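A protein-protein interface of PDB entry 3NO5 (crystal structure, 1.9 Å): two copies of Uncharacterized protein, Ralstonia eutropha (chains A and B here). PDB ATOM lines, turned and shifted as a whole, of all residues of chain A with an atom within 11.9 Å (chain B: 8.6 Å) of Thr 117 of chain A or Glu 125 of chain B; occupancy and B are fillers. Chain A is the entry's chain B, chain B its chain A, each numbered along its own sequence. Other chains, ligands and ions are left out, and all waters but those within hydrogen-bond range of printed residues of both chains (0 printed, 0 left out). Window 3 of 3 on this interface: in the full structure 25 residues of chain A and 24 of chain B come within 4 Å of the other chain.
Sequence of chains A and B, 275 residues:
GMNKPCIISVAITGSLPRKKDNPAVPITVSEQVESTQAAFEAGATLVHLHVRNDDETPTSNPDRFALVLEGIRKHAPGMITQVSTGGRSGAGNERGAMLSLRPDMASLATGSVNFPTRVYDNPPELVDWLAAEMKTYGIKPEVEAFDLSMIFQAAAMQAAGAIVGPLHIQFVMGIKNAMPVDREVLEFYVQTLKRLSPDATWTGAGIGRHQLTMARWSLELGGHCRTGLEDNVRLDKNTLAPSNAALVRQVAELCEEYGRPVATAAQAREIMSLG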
ATOM      1  N   SER A  15      -7.077   8.660 -27.850  1.00  0.00           N
ATOM      2  CA  SER A  15      -5.982   7.763 -27.466  1.00  0.00           C
ATOM      3  C   SER A  15      -6.472   6.567 -26.627  1.00  0.00           C
ATOM      4  O   SER A  15      -5.767   5.560 -26.533  1.00  0.00           O
ATOM      5  CB  SER A  15      -4.903   8.531 -26.708  1.00  0.00           C
ATOM      6  OG  SER A  15      -5.433   9.140 -25.541  1.00  0.00           O
ATOM      7  N   LEU A  16      -7.684   6.674 -26.033  1.00  0.00           N
ATOM      8  CA  LEU A  16      -8.227   5.628 -25.152  1.00  0.00           C
ATOM      9  C   LEU A  16      -9.234   4.657 -25.835  1.00  0.00           C
ATOM     10  O   LEU A  16      -9.145   3.450 -25.604  1.00  0.00           O
ATOM     11  CB  LEU A  16      -8.850   6.246 -23.879  1.00  0.00           C
ATOM     12  CG  LEU A  16      -7.880   6.966 -22.928  1.00  0.00           C
ATOM     13  CD1 LEU A  16      -8.636   7.767 -21.894  1.00  0.00           C
ATOM     14  CD2 LEU A  16      -6.926   5.972 -22.241  1.00  0.00           C
ATOM     15  N   GLY A  87      -0.241  13.497 -25.089  1.00  0.00           N
ATOM     16  CA  GLY A  87       0.725  12.437 -24.819  1.00  0.00           C
ATOM     17  C   GLY A  87       0.862  12.075 -23.354  1.00  0.00           C
ATOM     18  O   GLY A  87       0.281  12.734 -22.488  1.00  0.00           O
ATOM     19  N   ARG A  88       1.668  11.032 -23.061  1.00  0.00           N
ATOM     20  CA  ARG A  88       1.880  10.553 -21.692  1.00  0.00           C
ATOM     21  C   ARG A  88       2.862  11.441 -20.910  1.00  0.00           C
ATOM     22  O   ARG A  88       3.559  12.270 -21.503  1.00  0.00           O
ATOM     23  CB  ARG A  88       2.357   9.095 -21.702  1.00  0.00           C
ATOM     24  N   SER A  89       2.908  11.268 -19.566  1.00  0.00           N
ATOM     25  CA  SER A  89       3.795  12.040 -18.687  1.00  0.00           C
ATOM     26  C   SER A  89       5.257  11.671 -18.922  1.00  0.00           C
ATOM     27  O   SER A  89       5.615  10.491 -18.885  1.00  0.00           O
ATOM     28  CB  SER A  89       3.425  11.812 -17.224  1.00  0.00           C
ATOM     29  OG  SER A  89       2.094  12.225 -16.958  1.00  0.00           O
ATOM     30  N   VAL A 113      -3.269  19.419 -15.598  1.00  0.00           N
ATOM     31  CA  VAL A 113      -4.504  19.117 -14.874  1.00  0.00           C
ATOM     32  C   VAL A 113      -4.522  17.626 -14.505  1.00  0.00           C
ATOM     33  O   VAL A 113      -3.882  16.817 -15.182  1.00  0.00           O
ATOM     34  CB  VAL A 113      -5.762  19.520 -15.721  1.00  0.00           C
ATOM     35  CG1 VAL A 113      -5.941  18.599 -16.930  1.00  0.00           C
ATOM     36  CG2 VAL A 113      -7.025  19.548 -14.866  1.00  0.00           C
ATOM     37  N   ASN A 114      -5.235  17.265 -13.431  1.00  0.00           N
ATOM     38  CA  ASN A 114      -5.378  15.865 -13.054  1.00  0.00           C
ATOM     39  C   ASN A 114      -6.389  15.167 -13.942  1.00  0.00           C
ATOM     40  O   ASN A 114      -7.422  15.746 -14.279  1.00  0.00           O
ATOM     41  CB  ASN A 114      -5.766  15.724 -11.578  1.00  0.00           C
ATOM     42  CG  ASN A 114      -4.585  15.731 -10.633  1.00  0.00           C
ATOM     43  OD1 ASN A 114      -3.430  15.839 -11.043  1.00  0.00           O
ATOM     44  ND2 ASN A 114      -4.852  15.565  -9.349  1.00  0.00           N
ATOM     45  N   PHE A 115      -6.059  13.953 -14.380  1.00  0.00           N
ATOM     46  CA  PHE A 115      -6.940  13.118 -15.192  1.00  0.00           C
ATOM     47  C   PHE A 115      -7.477  11.950 -14.318  1.00  0.00           C
ATOM     48  O   PHE A 115      -7.132  11.878 -13.135  1.00  0.00           O
ATOM     49  CB  PHE A 115      -6.183  12.600 -16.442  1.00  0.00           C
ATOM     50  CG  PHE A 115      -6.436  13.398 -17.708  1.00  0.00           C
ATOM     51  CD1 PHE A 115      -6.858  14.728 -17.645  1.00  0.00           C
ATOM     52  CD2 PHE A 115      -6.220  12.834 -18.960  1.00  0.00           C
ATOM     53  CE1 PHE A 115      -7.091  15.460 -18.813  1.00  0.00           C
ATOM     54  CE2 PHE A 115      -6.447  13.572 -20.126  1.00  0.00           C
ATOM     55  CZ  PHE A 115      -6.883  14.878 -20.044  1.00  0.00           C
ATOM     56  N   PRO A 116      -8.375  11.067 -14.840  1.00  0.00           N
ATOM     57  CA  PRO A 116      -8.968  10.031 -13.965  1.00  0.00           C
ATOM     58  C   PRO A 116      -7.961   9.131 -13.239  1.00  0.00           C
ATOM     59  O   PRO A 116      -8.205   8.765 -12.089  1.00  0.00           O
ATOM     60  CB  PRO A 116      -9.858   9.228 -14.919  1.00  0.00           C
ATOM     61  CG  PRO A 116     -10.189  10.179 -16.011  1.00  0.00           C
ATOM     62  CD  PRO A 116      -8.962  11.027 -16.195  1.00  0.00           C
ATOM     63  N   THR A 117      -6.833   8.763 -13.906  1.00  0.00           N
ATOM     64  CA  THR A 117      -5.858   7.819 -13.326  1.00  0.00           C
ATOM     65  C   THR A 117      -4.436   8.400 -13.204  1.00  0.00           C
ATOM     66  O   THR A 117      -3.571   7.774 -12.580  1.00  0.00           O
ATOM     67  CB  THR A 117      -5.850   6.500 -14.125  1.00  0.00           C
ATOM     68  OG1 THR A 117      -5.479   6.776 -15.478  1.00  0.00           O
ATOM     69  CG2 THR A 117      -7.198   5.777 -14.083  1.00  0.00           C
ATOM     70  N   ARG A 118      -4.177   9.557 -13.830  1.00  0.00           N
ATOM     71  CA  ARG A 118      -2.833  10.153 -13.821  1.00  0.00           C
ATOM     72  C   ARG A 118      -2.894  11.680 -13.907  1.00  0.00           C
ATOM     73  O   ARG A 118      -3.978  12.250 -13.969  1.00  0.00           O
ATOM     74  CB  ARG A 118      -1.986   9.590 -14.993  1.00  0.00           C
ATOM     75  CG  ARG A 118      -2.493  10.023 -16.380  1.00  0.00           C
ATOM     76  CD  ARG A 118      -1.516   9.671 -17.484  1.00  0.00           C
ATOM     77  NE  ARG A 118      -1.929  10.230 -18.775  1.00  0.00           N
ATOM     78  CZ  ARG A 118      -1.368  11.299 -19.339  1.00  0.00           C
ATOM     79  NH1 ARG A 118      -0.352  11.916 -18.746  1.00  0.00           N
ATOM     80  NH2 ARG A 118      -1.804  11.744 -20.511  1.00  0.00           N
ATOM     81  N   VAL A 119      -1.723  12.333 -13.957  1.00  0.00           N
ATOM     82  CA  VAL A 119      -1.633  13.767 -14.188  1.00  0.00           C
ATOM     83  C   VAL A 119      -1.460  13.998 -15.680  1.00  0.00           C
ATOM     84  O   VAL A 119      -0.580  13.387 -16.291  1.00  0.00           O
ATOM     85  CB  VAL A 119      -0.453  14.409 -13.394  1.00  0.00           C
ATOM     86  CG1 VAL A 119      -0.336  15.907 -13.696  1.00  0.00           C
ATOM     87  CG2 VAL A 119      -0.597  14.168 -11.898  1.00  0.00           C
ATOM     88  N   TYR A 120      -2.277  14.881 -16.275  1.00  0.00           N
ATOM     89  CA  TYR A 120      -2.061  15.264 -17.661  1.00  0.00           C
ATOM     90  C   TYR A 120      -0.987  16.350 -17.693  1.00  0.00           C
ATOM     91  O   TYR A 120      -1.289  17.535 -17.521  1.00  0.00           O
ATOM     92  CB  TYR A 120      -3.369  15.725 -18.340  1.00  0.00           C
ATOM     93  CG  TYR A 120      -3.203  16.048 -19.816  1.00  0.00           C
ATOM     94  CD1 TYR A 120      -2.340  15.308 -20.622  1.00  0.00           C
ATOM     95  CD2 TYR A 120      -3.955  17.051 -20.418  1.00  0.00           C
ATOM     96  CE1 TYR A 120      -2.166  15.615 -21.971  1.00  0.00           C
ATOM     97  CE2 TYR A 120      -3.815  17.344 -21.777  1.00  0.00           C
ATOM     98  CZ  TYR A 120      -2.913  16.626 -22.548  1.00  0.00           C
ATOM     99  OH  TYR A 120      -2.769  16.904 -23.889  1.00  0.00           O
ATOM    100  N   ASP A 121       0.281  15.922 -17.774  1.00  0.00           N
ATOM    101  CA  ASP A 121       1.434  16.810 -17.700  1.00  0.00           C
ATOM    102  C   ASP A 121       1.657  17.606 -18.959  1.00  0.00           C
ATOM    103  O   ASP A 121       1.753  17.041 -20.050  1.00  0.00           O
ATOM    104  CB  ASP A 121       2.700  16.028 -17.330  1.00  0.00           C
ATOM    105  CG  ASP A 121       2.790  15.705 -15.860  1.00  0.00           C
ATOM    106  OD1 ASP A 121       3.004  16.637 -15.062  1.00  0.00           O
ATOM    107  OD2 ASP A 121       2.670  14.515 -15.507  1.00  0.00           O
ATOM    108  N   GLY A 174     -16.345  17.315 -17.775  1.00  0.00           N
ATOM    109  CA  GLY A 174     -16.810  15.947 -17.562  1.00  0.00           C
ATOM    110  C   GLY A 174     -15.723  14.929 -17.284  1.00  0.00           C
ATOM    111  O   GLY A 174     -16.025  13.755 -17.064  1.00  0.00           O
ATOM    112  N   ILE A 175     -14.447  15.359 -17.287  1.00  0.00           N
ATOM    113  CA  ILE A 175     -13.335  14.441 -16.995  1.00  0.00           C
ATOM    114  C   ILE A 175     -13.131  14.311 -15.485  1.00  0.00           C
ATOM    115  O   ILE A 175     -12.992  15.319 -14.796  1.00  0.00           O
ATOM    116  CB  ILE A 175     -12.023  14.864 -17.736  1.00  0.00           C
ATOM    117  CG1 ILE A 175     -12.223  14.851 -19.267  1.00  0.00           C
ATOM    118  CG2 ILE A 175     -10.836  13.972 -17.319  1.00  0.00           C
ATOM    119  CD1 ILE A 175     -11.091  15.504 -20.056  1.00  0.00           C
ATOM    120  N   LYS A 176     -13.107  13.061 -14.973  1.00  0.00           N
ATOM    121  CA  LYS A 176     -12.889  12.795 -13.550  1.00  0.00           C
ATOM    122  C   LYS A 176     -11.550  13.389 -13.087  1.00  0.00           C
ATOM    123  O   LYS A 176     -10.535  13.227 -13.771  1.00  0.00           O
ATOM    124  CB  LYS A 176     -12.935  11.284 -13.266  1.00  0.00           C
ATOM    125  CG  LYS A 176     -12.951  10.953 -11.783  1.00  0.00           C
ATOM    126  CD  LYS A 176     -12.757   9.476 -11.525  1.00  0.00           C
ATOM    127  CE  LYS A 176     -12.917   9.148 -10.057  1.00  0.00           C
ATOM    128  NZ  LYS A 176     -11.805   9.701  -9.239  1.00  0.00           N
ATOM    129  N   ASN A 177     -11.569  14.131 -11.945  1.00  0.00           N
ATOM    130  CA  ASN A 177     -10.392  14.788 -11.343  1.00  0.00           C
ATOM    131  C   ASN A 177     -10.016  16.111 -12.009  1.00  0.00           C
ATOM    132  O   ASN A 177      -9.191  16.854 -11.466  1.00  0.00           O
ATOM    133  CB  ASN A 177      -9.189  13.835 -11.243  1.00  0.00           C
ATOM    134  CG  ASN A 177      -9.459  12.625 -10.377  1.00  0.00           C
ATOM    135  OD1 ASN A 177     -10.186  12.694  -9.375  1.00  0.00           O
ATOM    136  ND2 ASN A 177      -8.864  11.491 -10.735  1.00  0.00           N
ATOM    137  N   ALA A 178     -10.636  16.425 -13.170  1.00  0.00           N
ATOM    138  CA  ALA A 178     -10.428  17.703 -13.850  1.00  0.00           C
ATOM    139  C   ALA A 178     -11.628  18.635 -13.570  1.00  0.00           C
ATOM    140  O   ALA A 178     -12.072  18.721 -12.428  1.00  0.00           O
ATOM    141  CB  ALA A 178     -10.255  17.479 -15.349  1.00  0.00           C
ATOM    142  N   MET A 179     -12.153  19.317 -14.597  1.00  0.00           N
ATOM    143  CA  MET A 179     -13.304  20.210 -14.410  1.00  0.00           C
ATOM    144  C   MET A 179     -14.615  19.457 -14.654  1.00  0.00           C
ATOM    145  O   MET A 179     -14.842  18.961 -15.760  1.00  0.00           O
ATOM    146  CB  MET A 179     -13.202  21.436 -15.339  1.00  0.00           C
ATOM    147  CG  MET A 179     -14.333  22.464 -15.135  1.00  0.00           C
ATOM    148  SD  MET A 179     -14.338  23.259 -13.357  1.00  0.00           S
ATOM    149  CE  MET A 179     -12.685  24.201 -13.430  1.00  0.00           C
ATOM    150  N   ILE A 207     -17.529  15.109 -22.159  1.00  0.00           N
ATOM    151  CA  ILE A 207     -17.118  13.703 -22.208  1.00  0.00           C
ATOM    152  C   ILE A 207     -18.272  12.791 -21.791  1.00  0.00           C
ATOM    153  O   ILE A 207     -19.024  13.129 -20.874  1.00  0.00           O
ATOM    154  CB  ILE A 207     -15.822  13.475 -21.350  1.00  0.00           C
ATOM    155  CG1 ILE A 207     -14.553  13.857 -22.146  1.00  0.00           C
ATOM    156  CG2 ILE A 207     -15.722  12.033 -20.836  1.00  0.00           C
ATOM    157  CD1 ILE A 207     -14.326  15.353 -22.343  1.00  0.00           C
ATOM    158  N   ALA B  91       8.019  12.601  -6.234  1.00  0.00           N
ATOM    159  CA  ALA B  91       7.961  12.283  -4.805  1.00  0.00           C
ATOM    160  C   ALA B  91       6.566  11.787  -4.430  1.00  0.00           C
ATOM    161  O   ALA B  91       5.566  12.378  -4.842  1.00  0.00           O
ATOM    162  CB  ALA B  91       8.321  13.508  -3.977  1.00  0.00           C
ATOM    163  N   GLY B  92       6.511  10.673  -3.714  1.00  0.00           N
ATOM    164  CA  GLY B  92       5.252  10.055  -3.324  1.00  0.00           C
ATOM    165  C   GLY B  92       4.894  10.276  -1.873  1.00  0.00           C
ATOM    166  O   GLY B  92       4.780  11.420  -1.423  1.00  0.00           O
ATOM    167  N   ASN B  93       4.769   9.161  -1.114  1.00  0.00           N
ATOM    168  CA  ASN B  93       4.387   9.139   0.312  1.00  0.00           C
ATOM    169  C   ASN B  93       5.329   9.946   1.213  1.00  0.00           C
ATOM    170  O   ASN B  93       4.926  10.349   2.312  1.00  0.00           O
ATOM    171  CB  ASN B  93       4.285   7.693   0.813  1.00  0.00           C
ATOM    172  CG  ASN B  93       5.531   6.858   0.557  1.00  0.00           C
ATOM    173  OD1 ASN B  93       6.634   7.169   1.029  1.00  0.00           O
ATOM    174  ND2 ASN B  93       5.365   5.747  -0.146  1.00  0.00           N
ATOM    175  N   ASN B 122       0.602  16.659  -8.359  1.00  0.00           N
ATOM    176  CA  ASN B 122      -0.141  16.120  -7.229  1.00  0.00           C
ATOM    177  C   ASN B 122      -1.045  14.995  -7.726  1.00  0.00           C
ATOM    178  O   ASN B 122      -2.239  15.218  -7.979  1.00  0.00           O
ATOM    179  CB  ASN B 122      -0.949  17.215  -6.537  1.00  0.00           C
ATOM    180  CG  ASN B 122      -0.092  18.267  -5.888  1.00  0.00           C
ATOM    181  OD1 ASN B 122       0.559  18.027  -4.867  1.00  0.00           O
ATOM    182  ND2 ASN B 122      -0.057  19.452  -6.479  1.00  0.00           N
ATOM    183  N   PRO B 123      -0.462  13.791  -8.000  1.00  0.00           N
ATOM    184  CA  PRO B 123      -1.274  12.694  -8.557  1.00  0.00           C
ATOM    185  C   PRO B 123      -2.522  12.397  -7.728  1.00  0.00           C
ATOM    186  O   PRO B 123      -2.498  12.549  -6.504  1.00  0.00           O
ATOM    187  CB  PRO B 123      -0.302  11.509  -8.572  1.00  0.00           C
ATOM    188  CG  PRO B 123       1.047  12.126  -8.615  1.00  0.00           C
ATOM    189  CD  PRO B 123       0.947  13.380  -7.810  1.00  0.00           C
ATOM    190  N   PRO B 124      -3.648  11.996  -8.381  1.00  0.00           N
ATOM    191  CA  PRO B 124      -4.883  11.713  -7.614  1.00  0.00           C
ATOM    192  C   PRO B 124      -4.667  10.711  -6.475  1.00  0.00           C
ATOM    193  O   PRO B 124      -5.242  10.882  -5.397  1.00  0.00           O
ATOM    194  CB  PRO B 124      -5.844  11.168  -8.675  1.00  0.00           C
ATOM    195  CG  PRO B 124      -5.344  11.729  -9.962  1.00  0.00           C
ATOM    196  CD  PRO B 124      -3.852  11.788  -9.831  1.00  0.00           C
ATOM    197  N   GLU B 125      -3.804   9.677  -6.707  1.00  0.00           N
ATOM    198  CA  GLU B 125      -3.495   8.669  -5.688  1.00  0.00           C
ATOM    199  C   GLU B 125      -2.788   9.294  -4.482  1.00  0.00           C
ATOM    200  O   GLU B 125      -3.055   8.904  -3.341  1.00  0.00           O
ATOM    201  CB  GLU B 125      -2.666   7.499  -6.285  1.00  0.00           C
ATOM    202  CG  GLU B 125      -1.367   7.915  -6.972  1.00  0.00           C
ATOM    203  CD  GLU B 125      -1.465   8.137  -8.472  1.00  0.00           C
ATOM    204  OE1 GLU B 125      -2.407   8.834  -8.916  1.00  0.00           O
ATOM    205  OE2 GLU B 125      -0.549   7.683  -9.194  1.00  0.00           O
ATOM    206  N   LEU B 126      -1.918  10.302  -4.729  1.00  0.00           N
ATOM    207  CA  LEU B 126      -1.205  11.008  -3.666  1.00  0.00           C
ATOM    208  C   LEU B 126      -2.162  11.916  -2.877  1.00  0.00           C
ATOM    209  O   LEU B 126      -2.101  11.944  -1.646  1.00  0.00           O
ATOM    210  CB  LEU B 126      -0.036  11.823  -4.247  1.00  0.00           C
ATOM    211  CG  LEU B 126       0.820  12.597  -3.231  1.00  0.00           C
ATOM    212  CD1 LEU B 126       1.511  11.649  -2.246  1.00  0.00           C
ATOM    213  CD2 LEU B 126       1.839  13.453  -3.931  1.00  0.00           C
ATOM    214  N   VAL B 127      -3.062  12.643  -3.590  1.00  0.00           N
ATOM    215  CA  VAL B 127      -4.076  13.506  -2.957  1.00  0.00           C
ATOM    216  C   VAL B 127      -4.950  12.669  -1.991  1.00  0.00           C
ATOM    217  O   VAL B 127      -5.147  13.068  -0.838  1.00  0.00           O
ATOM    218  CB  VAL B 127      -4.940  14.247  -4.023  1.00  0.00           C
ATOM    219  CG1 VAL B 127      -6.060  15.054  -3.367  1.00  0.00           C
ATOM    220  CG2 VAL B 127      -4.072  15.146  -4.906  1.00  0.00           C
ATOM    221  N   ASP B 128      -5.433  11.490  -2.461  1.00  0.00           N
ATOM    222  CA  ASP B 128      -6.246  10.573  -1.648  1.00  0.00           C
ATOM    223  C   ASP B 128      -5.475  10.085  -0.419  1.00  0.00           C
ATOM    224  O   ASP B 128      -6.023  10.073   0.686  1.00  0.00           O
ATOM    225  CB  ASP B 128      -6.711   9.361  -2.489  1.00  0.00           C
ATOM    226  CG  ASP B 128      -7.697   9.696  -3.592  1.00  0.00           C
ATOM    227  OD1 ASP B 128      -8.360  10.749  -3.495  1.00  0.00           O
ATOM    228  OD2 ASP B 128      -7.860   8.869  -4.513  1.00  0.00           O
ATOM    229  N   TRP B 129      -4.204   9.663  -0.615  1.00  0.00           N
ATOM    230  CA  TRP B 129      -3.374   9.140   0.475  1.00  0.00           C
ATOM    231  C   TRP B 129      -3.099  10.200   1.540  1.00  0.00           C
ATOM    232  O   TRP B 129      -3.266   9.928   2.724  1.00  0.00           O
ATOM    233  CB  TRP B 129      -2.061   8.551  -0.067  1.00  0.00           C
ATOM    234  CG  TRP B 129      -1.210   7.918   0.991  1.00  0.00           C
ATOM    235  CD1 TRP B 129      -1.310   6.646   1.472  1.00  0.00           C
ATOM    236  CD2 TRP B 129      -0.150   8.545   1.727  1.00  0.00           C
ATOM    237  NE1 TRP B 129      -0.377   6.441   2.462  1.00  0.00           N
ATOM    238  CE2 TRP B 129       0.356   7.588   2.631  1.00  0.00           C
ATOM    239  CE3 TRP B 129       0.426   9.828   1.706  1.00  0.00           C
ATOM    240  CZ2 TRP B 129       1.413   7.870   3.505  1.00  0.00           C
ATOM    241  CZ3 TRP B 129       1.467  10.107   2.580  1.00  0.00           C
ATOM    242  CH2 TRP B 129       1.950   9.134   3.465  1.00  0.00           C
ATOM    243  N   LEU B 130      -2.692  11.421   1.116  1.00  0.00           N
ATOM    244  CA  LEU B 130      -2.413  12.529   2.045  1.00  0.00           C
ATOM    245  C   LEU B 130      -3.647  12.888   2.878  1.00  0.00           C
ATOM    246  O   LEU B 130      -3.533  13.068   4.093  1.00  0.00           O
ATOM    247  CB  LEU B 130      -1.910  13.771   1.284  1.00  0.00           C
ATOM    248  CG  LEU B 130      -0.485  13.686   0.704  1.00  0.00           C
ATOM    249  CD1 LEU B 130      -0.208  14.854  -0.221  1.00  0.00           C
ATOM    250  CD2 LEU B 130       0.561  13.626   1.814  1.00  0.00           C
ATOM    251  N   ALA B 131      -4.833  12.960   2.228  1.00  0.00           N
ATOM    252  CA  ALA B 131      -6.097  13.265   2.914  1.00  0.00           C
ATOM    253  C   ALA B 131      -6.447  12.184   3.939  1.00  0.00           C
ATOM    254  O   ALA B 131      -6.880  12.507   5.047  1.00  0.00           O
ATOM    255  CB  ALA B 131      -7.221  13.405   1.902  1.00  0.00           C
ATOM    256  N   ALA B 132      -6.247  10.895   3.573  1.00  0.00           N
ATOM    257  CA  ALA B 132      -6.525   9.771   4.469  1.00  0.00           C
ATOM    258  C   ALA B 132      -5.584   9.779   5.686  1.00  0.00           C
ATOM    259  O   ALA B 132      -6.031   9.528   6.810  1.00  0.00           O
ATOM    260  CB  ALA B 132      -6.403   8.455   3.713  1.00  0.00           C
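Asn 114 of chain A touches Pro 124 of chain B. Phe 115 of chain A touches Pro 124 of chain B. Thr 117 of chain A touches Glu 125 of chain B (O to OE1, 3.99 Å). Pro 123 of chain B touches Val 119 of chain A (CA to CG2, 3.7 Å). Asn 177 of chain A touches Pro 124 of chain B.
Printed residues of chain A that touch a printed residue of chain B: Asn 114, Phe 115, Thr 117, Val 119 and Asn 177. Hydrophobic or aromatic side chains of chain A within 4 Å of the printed part of chain B: Val 119. Along chain A the printed residues that touch a printed residue of chain B span positions 114 to 177. Among the printed residues, no Asp or Glu carboxylate lies within 4 Å of a Lys or Arg side-chain nitrogen of the other chain.
The side-chain amide nitrogen (ND2) of Asn 114 of chain A sits at hydrogen-bond distance from the backbone carbonyl oxygen (O) of Asn 122 of chain B (3.0 Å).
The backbone carbonyl oxygen of Val 119 of chain A sits at hydrogen-bond distance from the side-chain hydroxyl of Ser 89 of chain A (3.0 Å). The backbone carbonyl oxygen (O) of Asn 114 of chain A is in hydrogen-bond range of the backbone NH (N) of Ala 178 of chain A, 3.5 Å away. ND2 of Asn 177 of chain A sits at hydrogen-bond distance from O of Phe 115 of chain A (3.0 Å). O of Pro 116 of chain A lies within hydrogen-bond range of ND2 of Asn 177 of chain A. The side-chain amide oxygen (OD1) of Asn 177 of chain A sits at hydrogen-bond distance from the side-chain amino group (NZ) of Lys 176 of chain A.
No position is printed for both chains. Of the 6 pairs that touch across the chains among the printed residues, none has its exchanged pair printed and touching as well.
Of the printed residues of chain B, Thr 117 of chain A touches Glu 125. Of the printed residues of chain A, Glu 125 of chain B touches Thr 117 (3.99 Å). No residue of chain B comes within 4 Å of Pro 116 of chain A. Pro 123 of chain B touches just one residue of chain A: Val 119. Printed residues of chain A within 4 Å of Pro 124 of chain B: Asn 114 (3.9 Å), Phe 115 (3.6 Å) and Asn 177 (3.6 Å). Of the printed residues of chain B, Val 119 of chain A touches Pro 123. Printed residues of chain B within 4 Å of Asn 177 of chain A: Pro 124 (3.6 Å). Ile 175 of chain A touches none of the printed residues of chain B. Ala 178 of chain A touches none of the printed residues of chain B.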
